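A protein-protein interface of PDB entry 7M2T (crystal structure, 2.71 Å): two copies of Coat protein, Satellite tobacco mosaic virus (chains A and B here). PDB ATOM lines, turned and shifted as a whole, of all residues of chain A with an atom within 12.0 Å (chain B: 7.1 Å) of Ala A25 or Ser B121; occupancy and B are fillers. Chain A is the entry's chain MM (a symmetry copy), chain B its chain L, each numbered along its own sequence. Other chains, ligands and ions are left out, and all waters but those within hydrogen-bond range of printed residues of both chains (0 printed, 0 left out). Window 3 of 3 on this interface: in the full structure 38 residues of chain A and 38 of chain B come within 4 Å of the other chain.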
ATOM      1  N   THR A  21      21.638 -36.933  12.633  1.00  0.00           N
ATOM      2  CA  THR A  21      20.702 -35.932  13.114  1.00  0.00           C
ATOM      3  C   THR A  21      21.141 -34.560  12.630  1.00  0.00           C
ATOM      4  O   THR A  21      22.315 -34.328  12.334  1.00  0.00           O
ATOM      5  CB  THR A  21      20.589 -35.936  14.646  1.00  0.00           C
ATOM      6  OG1 THR A  21      21.881 -35.712  15.223  1.00  0.00           O
ATOM      7  CG2 THR A  21      20.039 -37.263  15.141  1.00  0.00           C
ATOM      8  N   MET A  22      20.178 -33.649  12.563  1.00  0.00           N
ATOM      9  CA  MET A  22      20.435 -32.311  12.049  1.00  0.00           C
ATOM     10  C   MET A  22      21.185 -31.466  13.073  1.00  0.00           C
ATOM     11  O   MET A  22      20.951 -31.567  14.279  1.00  0.00           O
ATOM     12  CB  MET A  22      19.114 -31.644  11.670  1.00  0.00           C
ATOM     13  CG  MET A  22      19.245 -30.240  11.108  1.00  0.00           C
ATOM     14  SD  MET A  22      18.111 -29.950   9.737  1.00  0.00           S
ATOM     15  CE  MET A  22      16.520 -30.121  10.541  1.00  0.00           C
ATOM     16  N   ILE A  23      22.115 -30.648  12.583  1.00  0.00           N
ATOM     17  CA  ILE A  23      22.727 -29.574  13.355  1.00  0.00           C
ATOM     18  C   ILE A  23      22.150 -28.261  12.849  1.00  0.00           C
ATOM     19  O   ILE A  23      22.048 -28.046  11.634  1.00  0.00           O
ATOM     20  CB  ILE A  23      24.262 -29.568  13.228  1.00  0.00           C
ATOM     21  CG1 ILE A  23      24.872 -30.806  13.880  1.00  0.00           C
ATOM     22  CG2 ILE A  23      24.846 -28.299  13.835  1.00  0.00           C
ATOM     23  CD1 ILE A  23      26.348 -30.971  13.573  1.00  0.00           C
ATOM     24  N   ARG A  24      21.770 -27.384  13.774  1.00  0.00           N
ATOM     25  CA  ARG A  24      21.216 -26.079  13.412  1.00  0.00           C
ATOM     26  C   ARG A  24      22.333 -25.036  13.394  1.00  0.00           C
ATOM     27  O   ARG A  24      22.436 -24.160  14.252  1.00  0.00           O
ATOM     28  CB  ARG A  24      20.085 -25.699  14.363  1.00  0.00           C
ATOM     29  CG  ARG A  24      18.801 -26.462  14.085  1.00  0.00           C
ATOM     30  CD  ARG A  24      17.735 -26.212  15.136  1.00  0.00           C
ATOM     31  NE  ARG A  24      16.489 -26.885  14.789  1.00  0.00           N
ATOM     32  CZ  ARG A  24      16.259 -28.179  14.966  1.00  0.00           C
ATOM     33  NH1 ARG A  24      17.177 -28.980  15.483  1.00  0.00           N
ATOM     34  NH2 ARG A  24      15.081 -28.684  14.612  1.00  0.00           N
ATOM     35  N   ALA A  25      23.179 -25.159  12.373  1.00  0.00           N
ATOM     36  CA  ALA A  25      24.314 -24.262  12.217  1.00  0.00           C
ATOM     37  C   ALA A  25      23.846 -22.824  12.026  1.00  0.00           C
ATOM     38  O   ALA A  25      22.773 -22.561  11.474  1.00  0.00           O
ATOM     39  CB  ALA A  25      25.174 -24.694  11.029  1.00  0.00           C
ATOM     40  N   GLY A  26      24.667 -21.888  12.491  1.00  0.00           N
ATOM     41  CA  GLY A  26      24.339 -20.485  12.369  1.00  0.00           C
ATOM     42  C   GLY A  26      25.222 -19.765  11.374  1.00  0.00           C
ATOM     43  O   GLY A  26      25.308 -20.157  10.207  1.00  0.00           O
ATOM     44  N   SER A  27      25.887 -18.708  11.826  1.00  0.00           N
ATOM     45  CA  SER A  27      26.733 -17.924  10.947  1.00  0.00           C
ATOM     46  C   SER A  27      28.037 -18.662  10.668  1.00  0.00           C
ATOM     47  O   SER A  27      28.473 -19.524  11.438  1.00  0.00           O
ATOM     48  CB  SER A  27      27.022 -16.560  11.564  1.00  0.00           C
ATOM     49  OG  SER A  27      25.817 -15.942  11.974  1.00  0.00           O
ATOM     50  N   TYR A  28      28.659 -18.314   9.547  1.00  0.00           N
ATOM     51  CA  TYR A  28      29.930 -18.929   9.203  1.00  0.00           C
ATOM     52  C   TYR A  28      30.972 -18.567  10.261  1.00  0.00           C
ATOM     53  O   TYR A  28      31.161 -17.380  10.559  1.00  0.00           O
ATOM     54  CB  TYR A  28      30.393 -18.482   7.819  1.00  0.00           C
ATOM     55  CG  TYR A  28      31.600 -19.249   7.344  1.00  0.00           C
ATOM     56  CD1 TYR A  28      31.454 -20.443   6.649  1.00  0.00           C
ATOM     57  CD2 TYR A  28      32.882 -18.795   7.609  1.00  0.00           C
ATOM     58  CE1 TYR A  28      32.556 -21.155   6.222  1.00  0.00           C
ATOM     59  CE2 TYR A  28      33.991 -19.503   7.190  1.00  0.00           C
ATOM     60  CZ  TYR A  28      33.822 -20.677   6.495  1.00  0.00           C
ATOM     61  OH  TYR A  28      34.924 -21.376   6.076  1.00  0.00           O
ATOM     62  N   PRO A  29      31.659 -19.542  10.844  1.00  0.00           N
ATOM     63  CA  PRO A  29      32.526 -19.262  11.991  1.00  0.00           C
ATOM     64  C   PRO A  29      33.900 -18.774  11.555  1.00  0.00           C
ATOM     65  O   PRO A  29      34.248 -18.767  10.374  1.00  0.00           O
ATOM     66  CB  PRO A  29      32.625 -20.626  12.675  1.00  0.00           C
ATOM     67  CG  PRO A  29      32.570 -21.588  11.539  1.00  0.00           C
ATOM     68  CD  PRO A  29      31.669 -20.971  10.488  1.00  0.00           C
ATOM     69  N   LYS A  30      34.684 -18.358  12.545  1.00  0.00           N
ATOM     70  CA  LYS A  30      36.100 -18.127  12.306  1.00  0.00           C
ATOM     71  C   LYS A  30      36.787 -19.468  12.074  1.00  0.00           C
ATOM     72  O   LYS A  30      36.473 -20.465  12.731  1.00  0.00           O
ATOM     73  CB  LYS A  30      36.744 -17.404  13.488  1.00  0.00           C
ATOM     74  CG  LYS A  30      35.914 -16.281  14.082  1.00  0.00           C
ATOM     75  CD  LYS A  30      35.747 -15.113  13.129  1.00  0.00           C
ATOM     76  CE  LYS A  30      34.949 -13.995  13.788  1.00  0.00           C
ATOM     77  NZ  LYS A  30      34.502 -12.941  12.831  1.00  0.00           N
ATOM     78  N   VAL A  31      37.717 -19.502  11.121  1.00  0.00           N
ATOM     79  CA  VAL A  31      38.368 -20.741  10.720  1.00  0.00           C
ATOM     80  C   VAL A  31      39.870 -20.508  10.592  1.00  0.00           C
ATOM     81  O   VAL A  31      40.355 -19.375  10.577  1.00  0.00           O
ATOM     82  CB  VAL A  31      37.799 -21.300   9.397  1.00  0.00           C
ATOM     83  CG1 VAL A  31      36.321 -21.648   9.552  1.00  0.00           C
ATOM     84  CG2 VAL A  31      38.009 -20.307   8.268  1.00  0.00           C
ATOM     85  N   VAL B  78      29.305 -32.503   9.760  1.00  0.00           N
ATOM     86  CA  VAL B  78      29.424 -31.762   8.510  1.00  0.00           C
ATOM     87  C   VAL B  78      28.515 -30.545   8.586  1.00  0.00           C
ATOM     88  O   VAL B  78      27.321 -30.679   8.868  1.00  0.00           O
ATOM     89  CB  VAL B  78      29.045 -32.625   7.290  1.00  0.00           C
ATOM     90  CG1 VAL B  78      29.222 -31.836   6.007  1.00  0.00           C
ATOM     91  CG2 VAL B  78      29.863 -33.901   7.257  1.00  0.00           C
ATOM     92  N   ARG B  79      29.076 -29.365   8.340  1.00  0.00           N
ATOM     93  CA  ARG B  79      28.322 -28.121   8.268  1.00  0.00           C
ATOM     94  C   ARG B  79      28.616 -27.444   6.939  1.00  0.00           C
ATOM     95  O   ARG B  79      29.740 -27.516   6.433  1.00  0.00           O
ATOM     96  CB  ARG B  79      28.674 -27.183   9.426  1.00  0.00           C
ATOM     97  CG  ARG B  79      28.165 -27.637  10.783  1.00  0.00           C
ATOM     98  CD  ARG B  79      28.678 -26.730  11.889  1.00  0.00           C
ATOM     99  NE  ARG B  79      30.117 -26.873  12.083  1.00  0.00           N
ATOM    100  CZ  ARG B  79      30.883 -25.991  12.711  1.00  0.00           C
ATOM    101  NH1 ARG B  79      30.387 -24.867  13.201  1.00  0.00           N
ATOM    102  NH2 ARG B  79      32.181 -26.241  12.844  1.00  0.00           N
ATOM    103  N   ALA B  80      27.605 -26.789   6.373  1.00  0.00           N
ATOM    104  CA  ALA B  80      27.744 -26.163   5.068  1.00  0.00           C
ATOM    105  C   ALA B  80      27.076 -24.796   5.051  1.00  0.00           C
ATOM    106  O   ALA B  80      25.993 -24.609   5.614  1.00  0.00           O
ATOM    107  CB  ALA B  80      27.150 -27.050   3.966  1.00  0.00           C
ATOM    108  N   TRP B  81      27.738 -23.848   4.401  1.00  0.00           N
ATOM    109  CA  TRP B  81      27.197 -22.526   4.139  1.00  0.00           C
ATOM    110  C   TRP B  81      27.258 -22.254   2.643  1.00  0.00           C
ATOM    111  O   TRP B  81      28.169 -22.721   1.952  1.00  0.00           O
ATOM    112  CB  TRP B  81      27.982 -21.441   4.889  1.00  0.00           C
ATOM    113  CG  TRP B  81      27.864 -21.502   6.380  1.00  0.00           C
ATOM    114  CD1 TRP B  81      27.062 -20.727   7.169  1.00  0.00           C
ATOM    115  CD2 TRP B  81      28.584 -22.367   7.269  1.00  0.00           C
ATOM    116  NE1 TRP B  81      27.231 -21.063   8.489  1.00  0.00           N
ATOM    117  CE2 TRP B  81      28.160 -22.065   8.580  1.00  0.00           C
ATOM    118  CE3 TRP B  81      29.542 -23.367   7.085  1.00  0.00           C
ATOM    119  CZ2 TRP B  81      28.661 -22.728   9.698  1.00  0.00           C
ATOM    120  CZ3 TRP B  81      30.038 -24.022   8.196  1.00  0.00           C
ATOM    121  CH2 TRP B  81      29.596 -23.701   9.486  1.00  0.00           C
ATOM    122  N   THR B  82      26.279 -21.509   2.135  1.00  0.00           N
ATOM    123  CA  THR B  82      26.396 -21.003   0.775  1.00  0.00           C
ATOM    124  C   THR B  82      27.493 -19.949   0.732  1.00  0.00           C
ATOM    125  O   THR B  82      27.641 -19.144   1.657  1.00  0.00           O
ATOM    126  CB  THR B  82      25.071 -20.425   0.277  1.00  0.00           C
ATOM    127  OG1 THR B  82      24.560 -19.478   1.222  1.00  0.00           O
ATOM    128  CG2 THR B  82      24.050 -21.530   0.067  1.00  0.00           C
ATOM    129  N   SER B  92      18.936 -17.784  -0.521  1.00  0.00           N
ATOM    130  CA  SER B  92      19.852 -18.912  -0.633  1.00  0.00           C
ATOM    131  C   SER B  92      19.319 -20.130   0.115  1.00  0.00           C
ATOM    132  O   SER B  92      18.631 -20.011   1.131  1.00  0.00           O
ATOM    133  CB  SER B  92      21.229 -18.537  -0.088  1.00  0.00           C
ATOM    134  OG  SER B  92      21.692 -17.334  -0.676  1.00  0.00           O
ATOM    135  N   PHE B  93      19.638 -21.315  -0.404  1.00  0.00           N
ATOM    136  CA  PHE B  93      19.365 -22.558   0.301  1.00  0.00           C
ATOM    137  C   PHE B  93      20.494 -23.546   0.042  1.00  0.00           C
ATOM    138  O   PHE B  93      21.205 -23.466  -0.962  1.00  0.00           O
ATOM    139  CB  PHE B  93      18.015 -23.172  -0.104  1.00  0.00           C
ATOM    140  CG  PHE B  93      18.022 -23.846  -1.448  1.00  0.00           C
ATOM    141  CD1 PHE B  93      18.464 -25.153  -1.589  1.00  0.00           C
ATOM    142  CD2 PHE B  93      17.553 -23.180  -2.567  1.00  0.00           C
ATOM    143  CE1 PHE B  93      18.465 -25.773  -2.826  1.00  0.00           C
ATOM    144  CE2 PHE B  93      17.542 -23.797  -3.804  1.00  0.00           C
ATOM    145  CZ  PHE B  93      18.002 -25.095  -3.936  1.00  0.00           C
ATOM    146  N   VAL B  94      20.641 -24.500   0.956  1.00  0.00           N
ATOM    147  CA  VAL B  94      21.634 -25.559   0.821  1.00  0.00           C
ATOM    148  C   VAL B  94      21.067 -26.827   1.444  1.00  0.00           C
ATOM    149  O   VAL B  94      20.463 -26.783   2.522  1.00  0.00           O
ATOM    150  CB  VAL B  94      22.985 -25.155   1.460  1.00  0.00           C
ATOM    151  CG1 VAL B  94      22.822 -24.823   2.942  1.00  0.00           C
ATOM    152  CG2 VAL B  94      24.022 -26.246   1.260  1.00  0.00           C
ATOM    153  N   LEU B  96      21.910 -31.027   2.399  1.00  0.00           N
ATOM    154  CA  LEU B  96      22.928 -32.040   2.637  1.00  0.00           C
ATOM    155  C   LEU B  96      22.280 -33.414   2.697  1.00  0.00           C
ATOM    156  O   LEU B  96      21.294 -33.610   3.417  1.00  0.00           O
ATOM    157  CB  LEU B  96      23.689 -31.757   3.931  1.00  0.00           C
ATOM    158  CG  LEU B  96      24.585 -30.523   3.866  1.00  0.00           C
ATOM    159  CD1 LEU B  96      25.387 -30.378   5.145  1.00  0.00           C
ATOM    160  CD2 LEU B  96      25.503 -30.614   2.657  1.00  0.00           C
ATOM    161  N   GLU B 110      18.114 -29.363   5.123  1.00  0.00           N
ATOM    162  CA  GLU B 110      18.052 -28.160   4.306  1.00  0.00           C
ATOM    163  C   GLU B 110      17.972 -26.926   5.186  1.00  0.00           C
ATOM    164  O   GLU B 110      17.192 -26.888   6.144  1.00  0.00           O
ATOM    165  CB  GLU B 110      16.850 -28.202   3.358  1.00  0.00           C
ATOM    166  CG  GLU B 110      16.684 -26.943   2.530  1.00  0.00           C
ATOM    167  CD  GLU B 110      15.569 -27.057   1.518  1.00  0.00           C
ATOM    168  OE1 GLU B 110      15.335 -28.175   1.007  1.00  0.00           O
ATOM    169  OE2 GLU B 110      14.918 -26.029   1.241  1.00  0.00           O
ATOM    170  N   GLY B 111      18.778 -25.928   4.855  1.00  0.00           N
ATOM    171  CA  GLY B 111      18.676 -24.612   5.463  1.00  0.00           C
ATOM    172  C   GLY B 111      18.423 -23.570   4.391  1.00  0.00           C
ATOM    173  O   GLY B 111      18.942 -23.677   3.276  1.00  0.00           O
ATOM    174  N   ARG B 112      17.611 -22.574   4.727  1.00  0.00           N
ATOM    175  CA  ARG B 112      17.340 -21.455   3.841  1.00  0.00           C
ATOM    176  C   ARG B 112      17.678 -20.155   4.550  1.00  0.00           C
ATOM    177  O   ARG B 112      17.558 -20.050   5.772  1.00  0.00           O
ATOM    178  CB  ARG B 112      15.876 -21.427   3.391  1.00  0.00           C
ATOM    179  CG  ARG B 112      15.411 -22.736   2.787  1.00  0.00           C
ATOM    180  CD  ARG B 112      14.006 -22.649   2.219  1.00  0.00           C
ATOM    181  NE  ARG B 112      13.543 -23.964   1.790  1.00  0.00           N
ATOM    182  CZ  ARG B 112      12.334 -24.225   1.312  1.00  0.00           C
ATOM    183  NH1 ARG B 112      11.416 -23.280   1.189  1.00  0.00           N
ATOM    184  NH2 ARG B 112      12.038 -25.467   0.947  1.00  0.00           N
ATOM    185  N   ALA B 113      18.120 -19.175   3.773  1.00  0.00           N
ATOM    186  CA  ALA B 113      18.296 -17.833   4.298  1.00  0.00           C
ATOM    187  C   ALA B 113      16.941 -17.152   4.439  1.00  0.00           C
ATOM    188  O   ALA B 113      15.994 -17.445   3.703  1.00  0.00           O
ATOM    189  CB  ALA B 113      19.209 -17.010   3.389  1.00  0.00           C
ATOM    190  N   ARG B 119      23.909 -15.845   4.126  1.00  0.00           N
ATOM    191  CA  ARG B 119      24.139 -17.244   3.806  1.00  0.00           C
ATOM    192  C   ARG B 119      23.024 -18.125   4.359  1.00  0.00           C
ATOM    193  O   ARG B 119      22.409 -17.823   5.383  1.00  0.00           O
ATOM    194  CB  ARG B 119      25.473 -17.713   4.382  1.00  0.00           C
ATOM    195  CG  ARG B 119      26.683 -16.904   3.960  1.00  0.00           C
ATOM    196  CD  ARG B 119      27.890 -17.321   4.787  1.00  0.00           C
ATOM    197  NE  ARG B 119      29.096 -16.582   4.437  1.00  0.00           N
ATOM    198  CZ  ARG B 119      30.034 -17.032   3.615  1.00  0.00           C
ATOM    199  NH1 ARG B 119      29.922 -18.206   3.015  1.00  0.00           N
ATOM    200  NH2 ARG B 119      31.114 -16.287   3.395  1.00  0.00           N
ATOM    201  N   ALA B 120      22.769 -19.226   3.663  1.00  0.00           N
ATOM    202  CA  ALA B 120      22.009 -20.332   4.219  1.00  0.00           C
ATOM    203  C   ALA B 120      22.981 -21.335   4.827  1.00  0.00           C
ATOM    204  O   ALA B 120      24.145 -21.415   4.427  1.00  0.00           O
ATOM    205  CB  ALA B 120      21.151 -21.001   3.146  1.00  0.00           C
ATOM    206  N   SER B 121      22.507 -22.094   5.811  1.00  0.00           N
ATOM    207  CA  SER B 121      23.405 -23.033   6.467  1.00  0.00           C
ATOM    208  C   SER B 121      22.610 -24.186   7.054  1.00  0.00           C
ATOM    209  O   SER B 121      21.471 -24.017   7.498  1.00  0.00           O
ATOM    210  CB  SER B 121      24.228 -22.354   7.566  1.00  0.00           C
ATOM    211  OG  SER B 121      23.393 -21.853   8.593  1.00  0.00           O
ATOM    212  N   VAL B 122      23.239 -25.359   7.051  1.00  0.00           N
ATOM    213  CA  VAL B 122      22.670 -26.559   7.651  1.00  0.00           C
ATOM    214  C   VAL B 122      23.829 -27.491   7.956  1.00  0.00           C
ATOM    215  O   VAL B 122      24.921 -27.351   7.403  1.00  0.00           O
ATOM    216  CB  VAL B 122      21.639 -27.235   6.712  1.00  0.00           C
ATOM    217  CG1 VAL B 122      22.355 -28.039   5.639  1.00  0.00           C
ATOM    218  CG2 VAL B 122      20.679 -28.112   7.502  1.00  0.00           C
ATOM    219  N   GLY B 123      23.594 -28.454   8.838  1.00  0.00           N
ATOM    220  CA  GLY B 123      24.610 -29.430   9.148  1.00  0.00           C
ATOM    221  C   GLY B 123      23.966 -30.699   9.653  1.00  0.00           C
ATOM    222  O   GLY B 123      22.764 -30.741   9.925  1.00  0.00           O
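Among the printed residues, merely in contact across the chains: Ser A27 with Trp B81 (3.3 Å), Met A22 with Gly B123 (3.5 Å), Pro A29 with Trp B81 (3.6 Å) and Met A22 with Val B122 (3.9 Å).
The backbone NH of Ala B80 is in hydrogen-bond range of the backbone carbonyl oxygen of Val B122, at 2.9 Å.
Ala A25 touches just one residue of chain B: Ser B121 (3.0 Å).
Of the printed residues of chain B, Tyr A28 touches Trp B81.
Ala B80 touches none of the printed residues of chain A.
No residue of chain A comes within 4 Å of Thr B82.
No residue of chain A comes within 4 Å of Val B94.
No residue of chain A comes within 4 Å of Gly B111.
No residue of chain A comes within 4 Å of Ala B120.
Of the printed residues of chain A, Val B122 touches Met A22 (3.9 Å).
The nearest printed residue of chain A that does not touch Ser B121 is Ser A27 (5.2 Å).
The nearest printed residue of chain B that does not touch Ser A27 is Ser B121 (5.2 Å).
No position is printed for both chains.
Of the 9 pairs that touch across the chains among the printed residues, none has its exchanged pair printed and touching as well.
The indole nitrogen (NE1) of Trp B81 sits at hydrogen-bond distance from the backbone carbonyl oxygen (O) of Gly A26.
The backbone carbonyl oxygen of Ala A25 is in hydrogen-bond range of the side-chain hydroxyl of Ser B121 (3.0 Å).
The backbone carbonyl oxygen of Gly A26 lies within hydrogen-bond range of the side-chain hydroxyl of Ser B121, 3.0 Å away.
The backbone carbonyl oxygen (O) of Gly B123 is in hydrogen-bond range of the backbone NH (N) of Ile A23 (2.7 Å).
The indole nitrogen (NE1) of Trp B81 sits close to the backbone NH (N) of Tyr A28.
Of the 18 printed residues of chain B, 4 touch a printed residue of chain A.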
